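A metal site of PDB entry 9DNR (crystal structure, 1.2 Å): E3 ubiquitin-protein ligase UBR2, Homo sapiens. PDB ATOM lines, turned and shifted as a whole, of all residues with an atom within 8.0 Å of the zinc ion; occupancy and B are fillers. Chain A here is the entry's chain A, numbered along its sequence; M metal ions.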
ATOM      1  N   SER A  14     -30.182  -4.549  19.224  1.00  0.00           N
ATOM      2  CA  SER A  14     -29.286  -3.799  20.070  1.00  0.00           C
ATOM      3  C   SER A  14     -28.195  -4.743  20.545  1.00  0.00           C
ATOM      4  O   SER A  14     -28.319  -5.964  20.426  1.00  0.00           O
ATOM      5  CB  SER A  14     -30.038  -3.173  21.250  1.00  0.00           C
ATOM      6  OG  SER A  14     -29.236  -2.197  21.870  1.00  0.00           O
ATOM      7  N   CYS A  15     -27.102  -4.179  21.001  1.00  0.00           N
ATOM      8  CA  CYS A  15     -26.024  -4.946  21.601  1.00  0.00           C
ATOM      9  C   CYS A  15     -25.977  -4.632  23.088  1.00  0.00           C
ATOM     10  O   CYS A  15     -25.762  -3.481  23.474  1.00  0.00           O
ATOM     11  CB  CYS A  15     -24.681  -4.619  20.958  1.00  0.00           C
ATOM     12  SG  CYS A  15     -23.431  -5.680  21.705  1.00  0.00           S
ATOM     13  N   ARG A  16     -26.219  -5.648  23.920  1.00  0.00           N
ATOM     14  CA  ARG A  16     -26.205  -5.421  25.361  1.00  0.00           C
ATOM     15  C   ARG A  16     -24.814  -5.072  25.861  1.00  0.00           C
ATOM     16  O   ARG A  16     -24.691  -4.437  26.920  1.00  0.00           O
ATOM     17  CB  ARG A  16     -26.806  -6.624  26.081  1.00  0.00           C
ATOM     18  CG  ARG A  16     -28.264  -6.871  25.684  1.00  0.00           C
ATOM     19  CD  ARG A  16     -28.797  -8.192  26.209  1.00  0.00           C
ATOM     20  NE  ARG A  16     -28.671  -8.298  27.660  1.00  0.00           N
ATOM     21  CZ  ARG A  16     -28.627  -9.458  28.306  1.00  0.00           C
ATOM     22  NH1 ARG A  16     -28.717 -10.613  27.676  1.00  0.00           N
ATOM     23  NH2 ARG A  16     -28.483  -9.449  29.632  1.00  0.00           N
ATOM     24  N   ASP A  17     -23.768  -5.441  25.131  1.00  0.00           N
ATOM     25  CA  ASP A  17     -22.405  -5.109  25.516  1.00  0.00           C
ATOM     26  C   ASP A  17     -21.981  -3.715  25.091  1.00  0.00           C
ATOM     27  O   ASP A  17     -21.198  -3.068  25.805  1.00  0.00           O
ATOM     28  CB  ASP A  17     -21.437  -6.122  24.923  1.00  0.00           C
ATOM     29  CG  ASP A  17     -21.704  -7.547  25.406  1.00  0.00           C
ATOM     30  OD1 ASP A  17     -21.919  -7.729  26.629  1.00  0.00           O
ATOM     31  OD2 ASP A  17     -21.668  -8.478  24.580  1.00  0.00           O
ATOM     32  N   CYS A  18     -22.451  -3.215  23.935  1.00  0.00           N
ATOM     33  CA  CYS A  18     -21.902  -1.988  23.373  1.00  0.00           C
ATOM     34  C   CYS A  18     -22.860  -0.803  23.356  1.00  0.00           C
ATOM     35  O   CYS A  18     -22.404   0.333  23.218  1.00  0.00           O
ATOM     36  CB  CYS A  18     -21.376  -2.225  21.951  1.00  0.00           C
ATOM     37  SG  CYS A  18     -20.124  -3.558  21.845  1.00  0.00           S
ATOM     38  N   ALA A  19     -24.167  -1.042  23.454  1.00  0.00           N
ATOM     39  CA  ALA A  19     -25.116   0.052  23.314  1.00  0.00           C
ATOM     40  C   ALA A  19     -24.946   1.024  24.468  1.00  0.00           C
ATOM     41  O   ALA A  19     -24.821   0.634  25.632  1.00  0.00           O
ATOM     42  CB  ALA A  19     -26.549  -0.494  23.359  1.00  0.00           C
ATOM     43  N   LEU A  26     -29.747  -1.175  15.659  1.00  0.00           N
ATOM     44  CA  LEU A  26     -29.259  -1.361  14.299  1.00  0.00           C
ATOM     45  C   LEU A  26     -30.314  -2.093  13.507  1.00  0.00           C
ATOM     46  O   LEU A  26     -31.023  -2.964  14.034  1.00  0.00           O
ATOM     47  CB  LEU A  26     -27.992  -2.219  14.277  1.00  0.00           C
ATOM     48  CG  LEU A  26     -26.783  -1.633  14.984  1.00  0.00           C
ATOM     49  CD1 LEU A  26     -25.658  -2.657  15.040  1.00  0.00           C
ATOM     50  CD2 LEU A  26     -26.310  -0.380  14.289  1.00  0.00           C
ATOM     51  N   PHE A  31     -26.534  -4.772  11.585  1.00  0.00           N
ATOM     52  CA  PHE A  31     -26.237  -5.729  12.637  1.00  0.00           C
ATOM     53  C   PHE A  31     -25.429  -6.919  12.095  1.00  0.00           C
ATOM     54  O   PHE A  31     -24.399  -7.290  12.657  1.00  0.00           O
ATOM     55  CB  PHE A  31     -27.528  -6.202  13.287  1.00  0.00           C
ATOM     56  CG  PHE A  31     -27.339  -7.378  14.171  1.00  0.00           C
ATOM     57  CD1 PHE A  31     -26.734  -7.219  15.393  1.00  0.00           C
ATOM     58  CD2 PHE A  31     -27.760  -8.639  13.786  1.00  0.00           C
ATOM     59  CE1 PHE A  31     -26.529  -8.314  16.234  1.00  0.00           C
ATOM     60  CE2 PHE A  31     -27.576  -9.732  14.627  1.00  0.00           C
ATOM     61  CZ  PHE A  31     -26.960  -9.570  15.840  1.00  0.00           C
ATOM     62  N   SER A  34     -21.811  -6.196  11.470  1.00  0.00           N
ATOM     63  CA  SER A  34     -21.145  -5.512  12.560  1.00  0.00           C
ATOM     64  C   SER A  34     -20.467  -6.522  13.487  1.00  0.00           C
ATOM     65  O   SER A  34     -20.672  -7.729  13.425  1.00  0.00           O
ATOM     66  CB  SER A  34     -22.139  -4.693  13.398  1.00  0.00           C
ATOM     67  OG  SER A  34     -22.922  -5.520  14.251  1.00  0.00           O
ATOM     68  N   ILE A  35     -19.644  -5.971  14.380  1.00  0.00           N
ATOM     69  CA  ILE A  35     -19.018  -6.804  15.408  1.00  0.00           C
ATOM     70  C   ILE A  35     -20.031  -7.370  16.390  1.00  0.00           C
ATOM     71  O   ILE A  35     -19.758  -8.384  17.050  1.00  0.00           O
ATOM     72  CB  ILE A  35     -17.907  -5.993  16.105  1.00  0.00           C
ATOM     73  CG1 ILE A  35     -16.930  -6.920  16.819  1.00  0.00           C
ATOM     74  CG2 ILE A  35     -18.500  -4.950  17.039  1.00  0.00           C
ATOM     75  CD1 ILE A  35     -16.063  -7.736  15.880  1.00  0.00           C
ATOM     76  N   HIS A  36     -21.212  -6.762  16.488  1.00  0.00           N
ATOM     77  CA  HIS A  36     -22.162  -7.091  17.545  1.00  0.00           C
ATOM     78  C   HIS A  36     -22.890  -8.399  17.312  1.00  0.00           C
ATOM     79  O   HIS A  36     -23.516  -8.896  18.240  1.00  0.00           O
ATOM     80  CB  HIS A  36     -23.146  -5.947  17.738  1.00  0.00           C
ATOM     81  CG  HIS A  36     -22.465  -4.628  17.843  1.00  0.00           C
ATOM     82  ND1 HIS A  36     -21.656  -4.265  18.908  1.00  0.00           N
ATOM     83  CD2 HIS A  36     -22.402  -3.608  16.941  1.00  0.00           C
ATOM     84  CE1 HIS A  36     -21.165  -3.067  18.666  1.00  0.00           C
ATOM     85  NE2 HIS A  36     -21.599  -2.647  17.490  1.00  0.00           N
ATOM     86  N   ARG A  37     -22.816  -8.963  16.107  1.00  0.00           N
ATOM     87  CA  ARG A  37     -23.355 -10.302  15.902  1.00  0.00           C
ATOM     88  C   ARG A  37     -22.607 -11.364  16.682  1.00  0.00           C
ATOM     89  O   ARG A  37     -23.101 -12.485  16.814  1.00  0.00           O
ATOM     90  CB  ARG A  37     -23.384 -10.658  14.409  1.00  0.00           C
ATOM     91  CG  ARG A  37     -22.010 -10.847  13.786  1.00  0.00           C
ATOM     92  CD  ARG A  37     -22.133 -11.263  12.319  1.00  0.00           C
ATOM     93  NE  ARG A  37     -22.616 -12.634  12.212  1.00  0.00           N
ATOM     94  CZ  ARG A  37     -23.442 -13.077  11.266  1.00  0.00           C
ATOM     95  NH1 ARG A  37     -23.841 -12.293  10.280  1.00  0.00           N
ATOM     96  NH2 ARG A  37     -23.872 -14.329  11.315  1.00  0.00           N
ATOM     97  N   ASP A  38     -21.428 -11.046  17.204  1.00  0.00           N
ATOM     98  CA  ASP A  38     -20.642 -11.930  18.046  1.00  0.00           C
ATOM     99  C   ASP A  38     -20.783 -11.593  19.525  1.00  0.00           C
ATOM    100  O   ASP A  38     -20.102 -12.198  20.356  1.00  0.00           O
ATOM    101  CB  ASP A  38     -19.178 -11.876  17.612  1.00  0.00           C
ATOM    102  CG  ASP A  38     -18.973 -12.487  16.242  1.00  0.00           C
ATOM    103  OD1 ASP A  38     -19.641 -13.478  15.912  1.00  0.00           O
ATOM    104  OD2 ASP A  38     -18.137 -11.942  15.493  1.00  0.00           O
ATOM    105  N   HIS A  39     -21.651 -10.654  19.866  1.00  0.00           N
ATOM    106  CA  HIS A  39     -21.821 -10.158  21.223  1.00  0.00           C
ATOM    107  C   HIS A  39     -23.178 -10.598  21.744  1.00  0.00           C
ATOM    108  O   HIS A  39     -23.916 -11.333  21.083  1.00  0.00           O
ATOM    109  CB  HIS A  39     -21.719  -8.626  21.239  1.00  0.00           C
ATOM    110  CG  HIS A  39     -20.371  -8.112  20.855  1.00  0.00           C
ATOM    111  ND1 HIS A  39     -20.143  -6.773  20.616  1.00  0.00           N
ATOM    112  CD2 HIS A  39     -19.189  -8.741  20.674  1.00  0.00           C
ATOM    113  CE1 HIS A  39     -18.866  -6.607  20.326  1.00  0.00           C
ATOM    114  NE2 HIS A  39     -18.269  -7.780  20.354  1.00  0.00           N
ATOM    115  N   ARG A  40     -23.508 -10.141  22.950  1.00  0.00           N
ATOM    116  CA  ARG A  40     -24.817 -10.407  23.543  1.00  0.00           C
ATOM    117  C   ARG A  40     -25.813  -9.425  22.936  1.00  0.00           C
ATOM    118  O   ARG A  40     -26.004  -8.323  23.436  1.00  0.00           O
ATOM    119  CB  ARG A  40     -24.768 -10.235  25.060  1.00  0.00           C
ATOM    120  CG  ARG A  40     -23.989 -11.280  25.848  1.00  0.00           C
ATOM    121  CD  ARG A  40     -24.084 -11.001  27.358  1.00  0.00           C
ATOM    122  NE  ARG A  40     -23.745  -9.618  27.691  1.00  0.00           N
ATOM    123  CZ  ARG A  40     -24.393  -8.864  28.571  1.00  0.00           C
ATOM    124  NH1 ARG A  40     -25.386  -9.348  29.295  1.00  0.00           N
ATOM    125  NH2 ARG A  40     -24.037  -7.591  28.721  1.00  0.00           N
ATOM    126  N   TYR A  41     -26.474  -9.825  21.863  1.00  0.00           N
ATOM    127  CA  TYR A  41     -27.424  -8.940  21.198  1.00  0.00           C
ATOM    128  C   TYR A  41     -28.842  -9.236  21.666  1.00  0.00           C
ATOM    129  O   TYR A  41     -29.121 -10.274  22.262  1.00  0.00           O
ATOM    130  CB  TYR A  41     -27.322  -9.089  19.686  1.00  0.00           C
ATOM    131  CG  TYR A  41     -27.499 -10.512  19.192  1.00  0.00           C
ATOM    132  CD1 TYR A  41     -26.397 -11.328  18.975  1.00  0.00           C
ATOM    133  CD2 TYR A  41     -28.754 -11.029  18.932  1.00  0.00           C
ATOM    134  CE1 TYR A  41     -26.549 -12.627  18.522  1.00  0.00           C
ATOM    135  CE2 TYR A  41     -28.926 -12.327  18.478  1.00  0.00           C
ATOM    136  CZ  TYR A  41     -27.812 -13.116  18.272  1.00  0.00           C
ATOM    137  OH  TYR A  41     -27.973 -14.406  17.822  1.00  0.00           O
ATOM    138  N   TRP A  60     -22.691   3.839  20.506  1.00  0.00           N
ATOM    139  CA  TRP A  60     -21.991   2.566  20.638  1.00  0.00           C
ATOM    140  C   TRP A  60     -20.640   2.795  21.305  1.00  0.00           C
ATOM    141  O   TRP A  60     -19.854   3.647  20.871  1.00  0.00           O
ATOM    142  CB  TRP A  60     -21.759   1.908  19.272  1.00  0.00           C
ATOM    143  CG  TRP A  60     -23.030   1.824  18.505  1.00  0.00           C
ATOM    144  CD1 TRP A  60     -23.417   2.620  17.461  1.00  0.00           C
ATOM    145  CD2 TRP A  60     -24.115   0.929  18.758  1.00  0.00           C
ATOM    146  NE1 TRP A  60     -24.680   2.262  17.048  1.00  0.00           N
ATOM    147  CE2 TRP A  60     -25.132   1.231  17.834  1.00  0.00           C
ATOM    148  CE3 TRP A  60     -24.310  -0.101  19.673  1.00  0.00           C
ATOM    149  CZ2 TRP A  60     -26.342   0.538  17.817  1.00  0.00           C
ATOM    150  CZ3 TRP A  60     -25.498  -0.767  19.668  1.00  0.00           C
ATOM    151  CH2 TRP A  60     -26.504  -0.468  18.722  1.00  0.00           C
ATOM    152  N   LYS A  61     -20.363   1.996  22.343  1.00  0.00           N
ATOM    153  CA  LYS A  61     -19.079   2.106  23.045  1.00  0.00           C
ATOM    154  C   LYS A  61     -17.946   1.476  22.257  1.00  0.00           C
ATOM    155  O   LYS A  61     -16.783   1.777  22.502  1.00  0.00           O
ATOM    156  CB  LYS A  61     -19.181   1.501  24.448  1.00  0.00           C
ATOM    157  CG  LYS A  61     -20.297   2.094  25.298  1.00  0.00           C
ATOM    158  CD  LYS A  61     -20.368   1.485  26.679  1.00  0.00           C
ATOM    159  CE  LYS A  61     -20.627  -0.001  26.566  1.00  0.00           C
ATOM    160  NZ  LYS A  61     -21.203  -0.551  27.831  1.00  0.00           N
ATOM    161  N   GLU A  62     -18.285   0.592  21.305  1.00  0.00           N
ATOM    162  CA  GLU A  62     -17.351  -0.058  20.403  1.00  0.00           C
ATOM    163  C   GLU A  62     -18.136  -0.417  19.136  1.00  0.00           C
ATOM    164  O   GLU A  62     -19.349  -0.597  19.186  1.00  0.00           O
ATOM    165  CB  GLU A  62     -16.792  -1.325  21.071  1.00  0.00           C
ATOM    166  CG  GLU A  62     -16.331  -2.411  20.125  1.00  0.00           C
ATOM    167  CD  GLU A  62     -15.563  -3.517  20.823  1.00  0.00           C
ATOM    168  OE1 GLU A  62     -14.308  -3.449  20.860  1.00  0.00           O
ATOM    169  OE2 GLU A  62     -16.205  -4.456  21.325  1.00  0.00           O
ATOM    170  N   GLY A  63     -17.446  -0.491  18.013  1.00  0.00           N
ATOM    171  CA  GLY A  63     -18.067  -0.941  16.793  1.00  0.00           C
ATOM    172  C   GLY A  63     -19.233  -0.088  16.310  1.00  0.00           C
ATOM    173  O   GLY A  63     -20.307  -0.605  16.003  1.00  0.00           O
HETATM  174 ZN    ZN M   1     -21.389  -5.129  20.750  1.00  0.00          ZN
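ND1 of His 36 is bound to the zinc ion (2.1 Å). ND1 of His 39 binds the zinc ion (2.1 Å). SG of Cys 18 binds the zinc ion (2.3 Å). SG of Cys 15 binds the zinc ion (2.3 Å).
O of Glu 62 sits close to NE2 of His 36 (3.5 Å). The backbone carbonyl oxygen of Gly 63 lies within hydrogen-bond range of a ring nitrogen (NE2) of His 36 (2.8 Å). The backbone NH of His 36 sits at hydrogen-bond distance from the side-chain hydroxyl of Ser 34 (3.1 Å). N of Lys 61 lies within hydrogen-bond range of O of Cys 18. The backbone NH (N) of Asp 17 sits close to the side-chain sulfur (SG) of Cys 15, 3.5 Å away.
Four residues have an atom within 4 Å of the zinc ion: Cys 15, Cys 18, His 36 and His 39. Along chain A the residues within 4 Å of the zinc ion span positions 15 to 39.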
